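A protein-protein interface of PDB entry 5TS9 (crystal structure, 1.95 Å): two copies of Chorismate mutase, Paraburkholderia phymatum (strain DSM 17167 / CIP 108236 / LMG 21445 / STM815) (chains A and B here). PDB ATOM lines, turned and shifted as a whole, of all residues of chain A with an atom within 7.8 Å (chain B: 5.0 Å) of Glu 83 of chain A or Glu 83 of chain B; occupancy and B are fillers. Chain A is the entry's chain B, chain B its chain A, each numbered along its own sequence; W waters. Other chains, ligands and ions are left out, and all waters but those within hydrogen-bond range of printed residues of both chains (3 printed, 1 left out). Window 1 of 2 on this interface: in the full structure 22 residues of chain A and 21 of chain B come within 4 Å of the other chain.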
ATOM      1  N   LEU A  26      -8.824 -14.337   4.255  1.00  0.00           N
ATOM      2  CA  LEU A  26      -8.983 -15.288   5.347  1.00  0.00           C
ATOM      3  C   LEU A  26     -10.087 -14.861   6.306  1.00  0.00           C
ATOM      4  O   LEU A  26     -10.910 -15.679   6.738  1.00  0.00           O
ATOM      5  CB  LEU A  26      -7.657 -15.413   6.105  1.00  0.00           C
ATOM      6  CG  LEU A  26      -7.688 -16.404   7.253  1.00  0.00           C
ATOM      7  CD1 LEU A  26      -8.081 -17.753   6.673  1.00  0.00           C
ATOM      8  CD2 LEU A  26      -6.282 -16.460   7.912  1.00  0.00           C
ATOM      9  N   ALA A  29     -13.786 -15.763   6.659  1.00  0.00           N
ATOM     10  CA  ALA A  29     -14.229 -17.051   7.198  1.00  0.00           C
ATOM     11  C   ALA A  29     -15.157 -16.874   8.383  1.00  0.00           C
ATOM     12  O   ALA A  29     -16.053 -17.701   8.590  1.00  0.00           O
ATOM     13  CB  ALA A  29     -13.039 -17.907   7.619  1.00  0.00           C
ATOM     14  N   VAL A  43     -19.277 -27.098   5.619  1.00  0.00           N
ATOM     15  CA  VAL A  43     -18.139 -26.243   5.287  1.00  0.00           C
ATOM     16  C   VAL A  43     -17.627 -26.552   3.890  1.00  0.00           C
ATOM     17  O   VAL A  43     -17.288 -25.647   3.117  1.00  0.00           O
ATOM     18  CB  VAL A  43     -17.042 -26.407   6.349  1.00  0.00           C
ATOM     19  CG1 VAL A  43     -15.738 -25.791   5.885  1.00  0.00           C
ATOM     20  CG2 VAL A  43     -17.520 -25.743   7.647  1.00  0.00           C
ATOM     21  N   ASP A  76      -4.608 -23.093  -1.565  1.00  0.00           N
ATOM     22  CA  ASP A  76      -4.183 -22.785  -0.204  1.00  0.00           C
ATOM     23  C   ASP A  76      -5.123 -21.776   0.455  1.00  0.00           C
ATOM     24  O   ASP A  76      -5.373 -21.859   1.661  1.00  0.00           O
ATOM     25  CB  ASP A  76      -2.740 -22.269  -0.195  1.00  0.00           C
ATOM     26  CG  ASP A  76      -1.719 -23.357  -0.562  1.00  0.00           C
ATOM     27  OD1 ASP A  76      -1.994 -24.554  -0.326  1.00  0.00           O
ATOM     28  OD2 ASP A  76      -0.643 -23.019  -1.091  1.00  0.00           O
ATOM     29  N   GLN A  77      -5.640 -20.799  -0.300  1.00  0.00           N
ATOM     30  CA  GLN A  77      -6.569 -19.859   0.326  1.00  0.00           C
ATOM     31  C   GLN A  77      -7.829 -20.570   0.812  1.00  0.00           C
ATOM     32  O   GLN A  77      -8.316 -20.280   1.909  1.00  0.00           O
ATOM     33  CB  GLN A  77      -6.956 -18.721  -0.628  1.00  0.00           C
ATOM     34  CG  GLN A  77      -5.777 -17.928  -1.222  1.00  0.00           C
ATOM     35  CD  GLN A  77      -4.704 -17.574  -0.198  1.00  0.00           C
ATOM     36  OE1 GLN A  77      -4.925 -16.769   0.720  1.00  0.00           O
ATOM     37  NE2 GLN A  77      -3.523 -18.166  -0.360  1.00  0.00           N
ATOM     38  N   VAL A  78      -8.399 -21.461  -0.014  1.00  0.00           N
ATOM     39  CA  VAL A  78      -9.650 -22.107   0.379  1.00  0.00           C
ATOM     40  C   VAL A  78      -9.420 -23.074   1.533  1.00  0.00           C
ATOM     41  O   VAL A  78     -10.256 -23.186   2.437  1.00  0.00           O
ATOM     42  CB  VAL A  78     -10.327 -22.807  -0.817  1.00  0.00           C
ATOM     43  CG1 VAL A  78     -10.586 -21.814  -1.950  1.00  0.00           C
ATOM     44  CG2 VAL A  78      -9.515 -23.977  -1.288  1.00  0.00           C
ATOM     45  N   GLU A  79      -8.292 -23.769   1.547  1.00  0.00           N
ATOM     46  CA  GLU A  79      -8.018 -24.648   2.678  1.00  0.00           C
ATOM     47  C   GLU A  79      -7.850 -23.856   3.967  1.00  0.00           C
ATOM     48  O   GLU A  79      -8.331 -24.281   5.029  1.00  0.00           O
ATOM     49  CB  GLU A  79      -6.782 -25.506   2.404  1.00  0.00           C
ATOM     50  CG  GLU A  79      -7.015 -26.589   1.372  1.00  0.00           C
ATOM     51  CD  GLU A  79      -8.156 -27.535   1.754  1.00  0.00           C
ATOM     52  OE1 GLU A  79      -8.867 -27.995   0.838  1.00  0.00           O
ATOM     53  OE2 GLU A  79      -8.333 -27.818   2.967  1.00  0.00           O
ATOM     54  N   ALA A  80      -7.157 -22.714   3.911  1.00  0.00           N
ATOM     55  CA  ALA A  80      -7.015 -21.900   5.121  1.00  0.00           C
ATOM     56  C   ALA A  80      -8.378 -21.428   5.624  1.00  0.00           C
ATOM     57  O   ALA A  80      -8.641 -21.430   6.836  1.00  0.00           O
ATOM     58  CB  ALA A  80      -6.124 -20.692   4.843  1.00  0.00           C
ATOM     59  N   ASN A  81      -9.245 -21.001   4.701  1.00  0.00           N
ATOM     60  CA  ASN A  81     -10.570 -20.530   5.081  1.00  0.00           C
ATOM     61  C   ASN A  81     -11.375 -21.639   5.753  1.00  0.00           C
ATOM     62  O   ASN A  81     -12.024 -21.407   6.779  1.00  0.00           O
ATOM     63  CB  ASN A  81     -11.313 -20.008   3.847  1.00  0.00           C
ATOM     64  CG  ASN A  81     -12.177 -18.801   4.168  1.00  0.00           C
ATOM     65  OD1 ASN A  81     -13.317 -18.943   4.600  1.00  0.00           O
ATOM     66  ND2 ASN A  81     -11.628 -17.601   3.955  1.00  0.00           N
ATOM     67  N   LYS A  82     -11.341 -22.853   5.193  1.00  0.00           N
ATOM     68  CA  LYS A  82     -12.058 -23.965   5.823  1.00  0.00           C
ATOM     69  C   LYS A  82     -11.501 -24.272   7.205  1.00  0.00           C
ATOM     70  O   LYS A  82     -12.259 -24.642   8.114  1.00  0.00           O
ATOM     71  CB  LYS A  82     -11.998 -25.219   4.939  1.00  0.00           C
ATOM     72  CG  LYS A  82     -12.836 -25.089   3.663  1.00  0.00           C
ATOM     73  CD  LYS A  82     -12.836 -26.337   2.814  1.00  0.00           C
ATOM     74  CE  LYS A  82     -11.437 -26.835   2.492  1.00  0.00           C
ATOM     75  NZ  LYS A  82     -11.477 -27.886   1.408  1.00  0.00           N
ATOM     76  N   GLU A  83     -10.173 -24.177   7.374  1.00  0.00           N
ATOM     77  CA  GLU A  83      -9.593 -24.440   8.689  1.00  0.00           C
ATOM     78  C   GLU A  83     -10.186 -23.512   9.741  1.00  0.00           C
ATOM     79  O   GLU A  83     -10.519 -23.954  10.848  1.00  0.00           O
ATOM     80  CB  GLU A  83      -8.062 -24.313   8.633  1.00  0.00           C
ATOM     81  CG  GLU A  83      -7.427 -25.432   7.810  1.00  0.00           C
ATOM     82  CD  GLU A  83      -5.916 -25.308   7.589  1.00  0.00           C
ATOM     83  OE1 GLU A  83      -5.375 -26.182   6.882  1.00  0.00           O
ATOM     84  OE2 GLU A  83      -5.272 -24.373   8.118  1.00  0.00           O
ATOM     85  N   VAL A  84     -10.358 -22.236   9.415  1.00  0.00           N
ATOM     86  CA  VAL A  84     -10.965 -21.318  10.376  1.00  0.00           C
ATOM     87  C   VAL A  84     -12.436 -21.684  10.599  1.00  0.00           C
ATOM     88  O   VAL A  84     -12.904 -21.801  11.739  1.00  0.00           O
ATOM     89  CB  VAL A  84     -10.808 -19.861   9.903  1.00  0.00           C
ATOM     90  CG1 VAL A  84     -11.714 -18.939  10.746  1.00  0.00           C
ATOM     91  CG2 VAL A  84      -9.338 -19.419   9.980  1.00  0.00           C
ATOM     92  N   GLN A  85     -13.166 -21.942   9.516  1.00  0.00           N
ATOM     93  CA  GLN A  85     -14.593 -22.259   9.643  1.00  0.00           C
ATOM     94  C   GLN A  85     -14.831 -23.507  10.504  1.00  0.00           C
ATOM     95  O   GLN A  85     -15.728 -23.525  11.348  1.00  0.00           O
ATOM     96  CB  GLN A  85     -15.208 -22.471   8.253  1.00  0.00           C
ATOM     97  CG  GLN A  85     -15.131 -21.253   7.345  1.00  0.00           C
ATOM     98  CD  GLN A  85     -15.765 -21.536   5.995  1.00  0.00           C
ATOM     99  OE1 GLN A  85     -16.739 -22.285   5.900  1.00  0.00           O
ATOM    100  NE2 GLN A  85     -15.189 -20.970   4.946  1.00  0.00           N
ATOM    101  N   TYR A  86     -14.063 -24.573  10.286  1.00  0.00           N
ATOM    102  CA  TYR A  86     -14.280 -25.786  11.075  1.00  0.00           C
ATOM    103  C   TYR A  86     -14.056 -25.534  12.558  1.00  0.00           C
ATOM    104  O   TYR A  86     -14.831 -26.008  13.410  1.00  0.00           O
ATOM    105  CB  TYR A  86     -13.361 -26.908  10.601  1.00  0.00           C
ATOM    106  CG  TYR A  86     -13.844 -27.632   9.364  1.00  0.00           C
ATOM    107  CD1 TYR A  86     -15.061 -28.303   9.361  1.00  0.00           C
ATOM    108  CD2 TYR A  86     -13.058 -27.677   8.214  1.00  0.00           C
ATOM    109  CE1 TYR A  86     -15.497 -28.978   8.238  1.00  0.00           C
ATOM    110  CE2 TYR A  86     -13.475 -28.359   7.098  1.00  0.00           C
ATOM    111  CZ  TYR A  86     -14.701 -28.991   7.102  1.00  0.00           C
ATOM    112  OH  TYR A  86     -15.110 -29.670   5.983  1.00  0.00           O
ATOM    113  N   ALA A  87     -12.971 -24.829  12.897  1.00  0.00           N
ATOM    114  CA  ALA A  87     -12.686 -24.603  14.307  1.00  0.00           C
ATOM    115  C   ALA A  87     -13.737 -23.695  14.937  1.00  0.00           C
ATOM    116  O   ALA A  87     -14.205 -23.968  16.045  1.00  0.00           O
ATOM    117  CB  ALA A  87     -11.277 -24.023  14.476  1.00  0.00           C
ATOM    118  N   LEU A  88     -14.112 -22.603  14.254  1.00  0.00           N
ATOM    119  CA  LEU A  88     -15.148 -21.716  14.783  1.00  0.00           C
ATOM    120  C   LEU A  88     -16.440 -22.479  15.044  1.00  0.00           C
ATOM    121  O   LEU A  88     -17.037 -22.367  16.122  1.00  0.00           O
ATOM    122  CB  LEU A  88     -15.420 -20.553  13.819  1.00  0.00           C
ATOM    123  CG  LEU A  88     -14.348 -19.466  13.723  1.00  0.00           C
ATOM    124  CD1 LEU A  88     -14.731 -18.370  12.719  1.00  0.00           C
ATOM    125  CD2 LEU A  88     -14.035 -18.867  15.129  1.00  0.00           C
ATOM    126  N   LEU A  89     -16.881 -23.278  14.065  1.00  0.00           N
ATOM    127  CA  LEU A  89     -18.155 -23.971  14.215  1.00  0.00           C
ATOM    128  C   LEU A  89     -18.112 -24.935  15.385  1.00  0.00           C
ATOM    129  O   LEU A  89     -19.085 -25.060  16.132  1.00  0.00           O
ATOM    130  CB  LEU A  89     -18.504 -24.704  12.927  1.00  0.00           C
ATOM    131  CG  LEU A  89     -18.904 -23.773  11.781  1.00  0.00           C
ATOM    132  CD1 LEU A  89     -18.942 -24.546  10.484  1.00  0.00           C
ATOM    133  CD2 LEU A  89     -20.261 -23.183  12.082  1.00  0.00           C
ATOM    134  N   VAL A 156      -4.687 -17.045  17.832  1.00  0.00           N
ATOM    135  CA  VAL A 156      -3.853 -18.191  17.460  1.00  0.00           C
ATOM    136  C   VAL A 156      -4.471 -18.963  16.301  1.00  0.00           C
ATOM    137  O   VAL A 156      -3.761 -19.425  15.393  1.00  0.00           O
ATOM    138  CB  VAL A 156      -3.632 -19.100  18.681  1.00  0.00           C
ATOM    139  CG1 VAL A 156      -3.179 -20.486  18.244  1.00  0.00           C
ATOM    140  CG2 VAL A 156      -2.646 -18.440  19.692  1.00  0.00           C
ATOM    141  N   LEU A 157      -5.799 -19.126  16.318  1.00  0.00           N
ATOM    142  CA  LEU A 157      -6.480 -19.795  15.211  1.00  0.00           C
ATOM    143  C   LEU A 157      -6.275 -19.045  13.897  1.00  0.00           C
ATOM    144  O   LEU A 157      -5.947 -19.652  12.861  1.00  0.00           O
ATOM    145  CB  LEU A 157      -7.973 -19.933  15.521  1.00  0.00           C
ATOM    146  CG  LEU A 157      -8.842 -20.379  14.329  1.00  0.00           C
ATOM    147  CD1 LEU A 157      -8.463 -21.783  13.850  1.00  0.00           C
ATOM    148  CD2 LEU A 157     -10.343 -20.316  14.652  1.00  0.00           C
ATOM    149  N   ALA A 160      -2.573 -19.195  12.646  1.00  0.00           N
ATOM    150  CA  ALA A 160      -2.209 -20.521  12.140  1.00  0.00           C
ATOM    151  C   ALA A 160      -2.739 -20.738  10.731  1.00  0.00           C
ATOM    152  O   ALA A 160      -2.036 -21.276   9.865  1.00  0.00           O
ATOM    153  CB  ALA A 160      -2.739 -21.612  13.070  1.00  0.00           C
ATOM    154  N   ALA A 161      -3.981 -20.319  10.484  1.00  0.00           N
ATOM    155  CA  ALA A 161      -4.549 -20.438   9.163  1.00  0.00           C
ATOM    156  C   ALA A 161      -3.912 -19.448   8.199  1.00  0.00           C
ATOM    157  O   ALA A 161      -3.811 -19.730   6.998  1.00  0.00           O
ATOM    158  CB  ALA A 161      -6.074 -20.226   9.221  1.00  0.00           C
ATOM    159  N   LEU A 162      -3.474 -18.292   8.684  1.00  0.00           N
ATOM    160  CA  LEU A 162      -2.725 -17.414   7.783  1.00  0.00           C
ATOM    161  C   LEU A 162      -1.401 -18.062   7.395  1.00  0.00           C
ATOM    162  O   LEU A 162      -0.981 -17.971   6.241  1.00  0.00           O
ATOM    163  CB  LEU A 162      -2.505 -16.033   8.415  1.00  0.00           C
ATOM    164  CG  LEU A 162      -1.870 -14.935   7.525  1.00  0.00           C
ATOM    165  CD1 LEU A 162      -2.676 -14.715   6.247  1.00  0.00           C
ATOM    166  CD2 LEU A 162      -1.776 -13.628   8.290  1.00  0.00           C
ATOM    167  N   ASP A 163      -0.747 -18.771   8.327  1.00  0.00           N
ATOM    168  CA  ASP A 163       0.442 -19.540   7.935  1.00  0.00           C
ATOM    169  C   ASP A 163       0.104 -20.586   6.872  1.00  0.00           C
ATOM    170  O   ASP A 163       0.947 -20.907   6.016  1.00  0.00           O
ATOM    171  CB  ASP A 163       1.066 -20.235   9.142  1.00  0.00           C
ATOM    172  CG  ASP A 163       1.903 -19.280  10.019  1.00  0.00           C
ATOM    173  OD1 ASP A 163       2.541 -18.359   9.457  1.00  0.00           O
ATOM    174  OD2 ASP A 163       1.950 -19.480  11.262  1.00  0.00           O
ATOM    175  N   ARG A 164      -1.114 -21.134   6.924  1.00  0.00           N
ATOM    176  CA  ARG A 164      -1.553 -22.095   5.914  1.00  0.00           C
ATOM    177  C   ARG A 164      -1.782 -21.419   4.565  1.00  0.00           C
ATOM    178  O   ARG A 164      -1.483 -22.004   3.511  1.00  0.00           O
ATOM    179  CB  ARG A 164      -2.835 -22.795   6.390  1.00  0.00           C
ATOM    180  CG  ARG A 164      -3.422 -23.784   5.377  1.00  0.00           C
ATOM    181  CD  ARG A 164      -2.548 -25.037   5.281  1.00  0.00           C
ATOM    182  NE  ARG A 164      -3.051 -26.026   4.321  1.00  0.00           N
ATOM    183  CZ  ARG A 164      -2.873 -25.944   3.003  1.00  0.00           C
ATOM    184  NH1 ARG A 164      -2.227 -24.907   2.478  1.00  0.00           N
ATOM    185  NH2 ARG A 164      -3.350 -26.889   2.203  1.00  0.00           N
ATOM    186  N   ALA A 165      -2.318 -20.192   4.576  1.00  0.00           N
ATOM    187  CA  ALA A 165      -2.629 -19.472   3.331  1.00  0.00           C
ATOM    188  C   ALA A 165      -1.368 -19.095   2.545  1.00  0.00           C
ATOM    189  O   ALA A 165      -1.365 -19.155   1.307  1.00  0.00           O
ATOM    190  CB  ALA A 165      -3.432 -18.206   3.630  1.00  0.00           C
ATOM    191  N   GLU B  79      -4.748 -33.023   5.582  1.00  0.00           N
ATOM    192  CA  GLU B  79      -4.852 -31.562   5.649  1.00  0.00           C
ATOM    193  C   GLU B  79      -4.708 -31.056   7.078  1.00  0.00           C
ATOM    194  O   GLU B  79      -4.109 -30.005   7.312  1.00  0.00           O
ATOM    195  CB  GLU B  79      -6.184 -31.084   5.060  1.00  0.00           C
ATOM    196  CG  GLU B  79      -6.337 -31.338   3.575  1.00  0.00           C
ATOM    197  CD  GLU B  79      -5.311 -30.593   2.754  1.00  0.00           C
ATOM    198  OE1 GLU B  79      -4.966 -29.450   3.120  1.00  0.00           O
ATOM    199  OE2 GLU B  79      -4.844 -31.144   1.745  1.00  0.00           O
ATOM    200  N   ALA B  80      -5.278 -31.768   8.055  1.00  0.00           N
ATOM    201  CA  ALA B  80      -5.099 -31.317   9.434  1.00  0.00           C
ATOM    202  C   ALA B  80      -3.628 -31.413   9.832  1.00  0.00           C
ATOM    203  O   ALA B  80      -3.095 -30.536  10.522  1.00  0.00           O
ATOM    204  CB  ALA B  80      -5.968 -32.147  10.382  1.00  0.00           C
ATOM    205  N   ASN B  81      -2.960 -32.464   9.375  1.00  0.00           N
ATOM    206  CA  ASN B  81      -1.543 -32.636   9.680  1.00  0.00           C
ATOM    207  C   ASN B  81      -0.711 -31.508   9.072  1.00  0.00           C
ATOM    208  O   ASN B  81       0.164 -30.941   9.735  1.00  0.00           O
ATOM    209  CB  ASN B  81      -1.094 -34.010   9.179  1.00  0.00           C
ATOM    210  CG  ASN B  81      -0.039 -34.640  10.080  1.00  0.00           C
ATOM    211  OD1 ASN B  81       1.150 -34.336   9.967  1.00  0.00           O
ATOM    212  ND2 ASN B  81      -0.472 -35.509  10.979  1.00  0.00           N
ATOM    213  N   LYS B  82      -0.974 -31.156   7.812  1.00  0.00           N
ATOM    214  CA  LYS B  82      -0.269 -30.022   7.211  1.00  0.00           C
ATOM    215  C   LYS B  82      -0.582 -28.708   7.931  1.00  0.00           C
ATOM    216  O   LYS B  82       0.300 -27.866   8.082  1.00  0.00           O
ATOM    217  CB  LYS B  82      -0.603 -29.918   5.719  1.00  0.00           C
ATOM    218  CG  LYS B  82      -0.239 -31.203   4.942  1.00  0.00           C
ATOM    219  CD  LYS B  82      -0.346 -31.031   3.428  1.00  0.00           C
ATOM    220  CE  LYS B  82      -1.791 -30.853   3.010  1.00  0.00           C
ATOM    221  NZ  LYS B  82      -1.883 -30.750   1.496  1.00  0.00           N
ATOM    222  N   GLU B  83      -1.831 -28.506   8.371  1.00  0.00           N
ATOM    223  CA  GLU B  83      -2.175 -27.310   9.147  1.00  0.00           C
ATOM    224  C   GLU B  83      -1.227 -27.121  10.326  1.00  0.00           C
ATOM    225  O   GLU B  83      -0.718 -26.020  10.579  1.00  0.00           O
ATOM    226  CB  GLU B  83      -3.619 -27.421   9.647  1.00  0.00           C
ATOM    227  CG  GLU B  83      -4.053 -26.316  10.579  1.00  0.00           C
ATOM    228  CD  GLU B  83      -5.545 -26.378  10.933  1.00  0.00           C
ATOM    229  OE1 GLU B  83      -6.030 -25.466  11.621  1.00  0.00           O
ATOM    230  OE2 GLU B  83      -6.235 -27.334  10.524  1.00  0.00           O
ATOM    231  N   VAL B  84      -0.989 -28.194  11.069  1.00  0.00           N
ATOM    232  CA  VAL B  84      -0.076 -28.115  12.201  1.00  0.00           C
ATOM    233  C   VAL B  84       1.346 -27.859  11.710  1.00  0.00           C
ATOM    234  O   VAL B  84       2.040 -26.979  12.221  1.00  0.00           O
ATOM    235  CB  VAL B  84      -0.163 -29.394  13.050  1.00  0.00           C
ATOM    236  CG1 VAL B  84       0.907 -29.404  14.143  1.00  0.00           C
ATOM    237  CG2 VAL B  84      -1.551 -29.494  13.686  1.00  0.00           C
ATOM    238  N   GLN B  85       1.789 -28.603  10.694  1.00  0.00           N
ATOM    239  CA  GLN B  85       3.167 -28.468  10.233  1.00  0.00           C
ATOM    240  C   GLN B  85       3.460 -27.044   9.762  1.00  0.00           C
ATOM    241  O   GLN B  85       4.501 -26.472  10.102  1.00  0.00           O
ATOM    242  CB  GLN B  85       3.469 -29.454   9.104  1.00  0.00           C
ATOM    243  CG  GLN B  85       3.464 -30.916   9.492  1.00  0.00           C
ATOM    244  CD  GLN B  85       3.739 -31.805   8.295  1.00  0.00           C
ATOM    245  OE1 GLN B  85       4.679 -31.559   7.529  1.00  0.00           O
ATOM    246  NE2 GLN B  85       2.928 -32.854   8.127  1.00  0.00           N
ATOM    247  N   TYR B  86       2.581 -26.472   8.938  1.00  0.00           N
ATOM    248  CA  TYR B  86       2.846 -25.126   8.433  1.00  0.00           C
ATOM    249  C   TYR B  86       2.918 -24.120   9.581  1.00  0.00           C
ATOM    250  O   TYR B  86       3.750 -23.207   9.565  1.00  0.00           O
ATOM    251  CB  TYR B  86       1.764 -24.694   7.443  1.00  0.00           C
ATOM    252  CG  TYR B  86       1.890 -25.246   6.043  1.00  0.00           C
ATOM    253  CD1 TYR B  86       3.040 -25.013   5.274  1.00  0.00           C
ATOM    254  CD2 TYR B  86       0.844 -25.956   5.469  1.00  0.00           C
ATOM    255  CE1 TYR B  86       3.141 -25.496   3.970  1.00  0.00           C
ATOM    256  CE2 TYR B  86       0.928 -26.451   4.184  1.00  0.00           C
ATOM    257  CZ  TYR B  86       2.085 -26.213   3.427  1.00  0.00           C
ATOM    258  OH  TYR B  86       2.187 -26.726   2.148  1.00  0.00           O
ATOM    259  N   ALA B  87       2.030 -24.255  10.566  1.00  0.00           N
ATOM    260  CA  ALA B  87       1.986 -23.293  11.669  1.00  0.00           C
ATOM    261  C   ALA B  87       3.221 -23.413  12.551  1.00  0.00           C
ATOM    262  O   ALA B  87       3.820 -22.400  12.940  1.00  0.00           O
ATOM    263  CB  ALA B  87       0.720 -23.493  12.502  1.00  0.00           C
ATOM    264  N   LEU B 157      -3.744 -24.567  18.743  1.00  0.00           N
ATOM    265  CA  LEU B 157      -3.407 -24.989  17.385  1.00  0.00           C
ATOM    266  C   LEU B 157      -3.835 -26.429  17.127  1.00  0.00           C
ATOM    267  O   LEU B 157      -4.434 -26.740  16.089  1.00  0.00           O
ATOM    268  CB  LEU B 157      -1.899 -24.856  17.143  1.00  0.00           C
ATOM    269  CG  LEU B 157      -1.332 -25.536  15.883  1.00  0.00           C
ATOM    270  CD1 LEU B 157      -1.919 -24.945  14.579  1.00  0.00           C
ATOM    271  CD2 LEU B 157       0.223 -25.467  15.828  1.00  0.00           C
ATOM    272  N   ALA B 160      -7.650 -26.855  17.089  1.00  0.00           N
ATOM    273  CA  ALA B 160      -8.178 -26.342  15.825  1.00  0.00           C
ATOM    274  C   ALA B 160      -7.987 -27.356  14.709  1.00  0.00           C
ATOM    275  O   ALA B 160      -8.908 -27.613  13.923  1.00  0.00           O
ATOM    276  CB  ALA B 160      -7.505 -25.018  15.466  1.00  0.00           C
ATOM    277  N   ALA B 161      -6.808 -27.968  14.642  1.00  0.00           N
ATOM    278  CA  ALA B 161      -6.541 -28.941  13.598  1.00  0.00           C
ATOM    279  C   ALA B 161      -7.222 -30.274  13.884  1.00  0.00           C
ATOM    280  O   ALA B 161      -7.546 -31.015  12.944  1.00  0.00           O
ATOM    281  CB  ALA B 161      -5.021 -29.115  13.422  1.00  0.00           C
ATOM    282  N   ARG B 164     -10.407 -29.815  12.309  1.00  0.00           N
ATOM    283  CA  ARG B 164     -10.285 -30.041  10.872  1.00  0.00           C
ATOM    284  C   ARG B 164     -10.295 -31.532  10.560  1.00  0.00           C
ATOM    285  O   ARG B 164     -10.909 -31.969   9.575  1.00  0.00           O
ATOM    286  CB  ARG B 164      -8.994 -29.384  10.347  1.00  0.00           C
ATOM    287  CG  ARG B 164      -8.704 -29.615   8.848  1.00  0.00           C
ATOM    288  CD  ARG B 164      -9.697 -28.827   7.980  1.00  0.00           C
ATOM    289  NE  ARG B 164      -9.517 -29.009   6.539  1.00  0.00           N
ATOM    290  CZ  ARG B 164      -9.982 -30.055   5.865  1.00  0.00           C
ATOM    291  NH1 ARG B 164     -10.630 -31.023   6.513  1.00  0.00           N
ATOM    292  NH2 ARG B 164      -9.787 -30.143   4.549  1.00  0.00           N
HETATM  293  O   HOH W   1     -12.256 -30.595   2.121  1.00  0.00           O
HETATM  294  O   HOH W   2       0.083 -26.413   0.132  1.00  0.00           O
HETATM  295  O   HOH W   3      -1.765 -23.968   9.217  1.00  0.00           O
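The guanidinium group (NH2) of Arg 164 of chain B lies within salt-bridge range of the side-chain carboxylate (OE2) of Glu 79 of chain A, at 3.2 Å. The guanidinium group (NH2) of Arg 164 of chain A lies within salt-bridge range of the side-chain carboxylate (OE1) of Glu 79 of chain B, 3.2 Å away.
The side-chain amino group (NZ) of Lys 82 of chain A is in salt-bridge range of the side-chain carboxylate (OE1) of Glu 79 of chain A, 2.7 Å away. The guanidinium group (NE) of Arg 164 of chain A lies within salt-bridge range of the side-chain carboxylate (OE1) of Glu 83 of chain A (3.5 Å). The side-chain carboxylate (OE2) of Glu 79 of chain B lies within salt-bridge range of the side-chain amino group (NZ) of Lys 82 of chain B (3.0 Å). The side-chain carboxylate (OD1) of Asp 76 of chain A lies within salt-bridge range of the guanidinium group (NH1) of Arg 164 of chain A, 2.8 Å away.
Glu 79 of chain A touches Glu 79 of chain B (OE2 to OE1, 3.7 Å). Glu 83 of chain B touches Glu 83 of chain A. CD2 of Tyr 86 of chain A touches CD of Arg 164 of chain B, 3.6 Å away. CB of Ala 160 of chain B touches CD1 of Leu 157 of chain A, at 3.7 Å. Ala 160 of chain A touches Ala 87 of chain B. CB of Ala 160 of chain A touches CD1 of Leu 157 of chain B, at 3.7 Å. Ala 87 of chain B touches Asp 163 of chain A (CA to OD2, 3.8 Å). Arg 164 of chain A touches Tyr 86 of chain B.
Val 78 of chain A touches none of the printed residues of chain B. Of the printed residues of chain B, Glu 83 of chain A touches Glu 83 (3.4 Å). Printed residues of chain B within 4 Å of Leu 157 of chain A: Ala 160. Printed residues of chain B within 4 Å of Ala 160 of chain A: Ala 87 and Leu 157. Asn 81 of chain B touches none of the printed residues of chain A. Printed residues of chain A within 4 Å of Glu 83 of chain B: Glu 83. Printed residues of chain A within 4 Å of Tyr 86 of chain B: Arg 164. Printed residues of chain A within 4 Å of Ala 87 of chain B: Ala 160 (3.98 Å) and Asp 163 (3.8 Å). The nearest printed residue of chain A that does not touch Tyr 86 of chain B is Asp 163 of chain A (4.03 Å).
Printed residues of chain B that touch a printed residue of chain A: Glu 79, Glu 83, Tyr 86, Ala 87, Leu 157, Ala 160 and Arg 164. Along chain B the printed residues that touch a printed residue of chain A span positions 79 to 164. Hydrophobic or aromatic side chains of chain A within 4 Å of the printed part of chain B: Tyr 86, Leu 157 and Ala 160. Among the printed residues, 10 pairs touch across the chains. Among the printed residues, Asp or Glu carboxylates within 4 Å of a Lys or Arg side-chain nitrogen of the other chain: Glu 79 of chain A with Arg 164 of chain B and Arg 164 of chain A with Glu 79 of chain B.
Glu 79 of chain A touches Arg 164 of chain B, and with the chains exchanged Arg 164 of chain A touches Glu 79 of chain B. Glu 83 of chain B touches its own counterpart, Glu 83 of chain A. Leu 157 of chain A touches Ala 160 of chain B, and with the chains exchanged Ala 160 of chain A touches Leu 157 of chain B. Ala 160 of chain A touches Ala 87 of chain B, but with the chains exchanged Ala 87 of chain A does not touch Ala 160 of chain B (4.02 Å). 13 positions are printed for both chains. Of the 10 pairs that touch across the chains among the printed residues, 8 have their exchanged pair printed and touching as well.
Water W3 lies within hydrogen-bond range of the backbone carbonyl oxygen of Glu 83 of chain B (2.7 Å) and the backbone carbonyl oxygen of Ala 160 of chain A (2.8 Å). Water W2 lies within hydrogen-bond range of the side-chain carboxylate (OD1) of Asp 76 of chain A (2.8 Å) and the side-chain hydroxyl (OH) of Tyr 86 of chain B (2.9 Å). Water W1 bridges the side-chain amino group of Lys 82 of chain A and the guanidinium group of Arg 164 of chain B.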
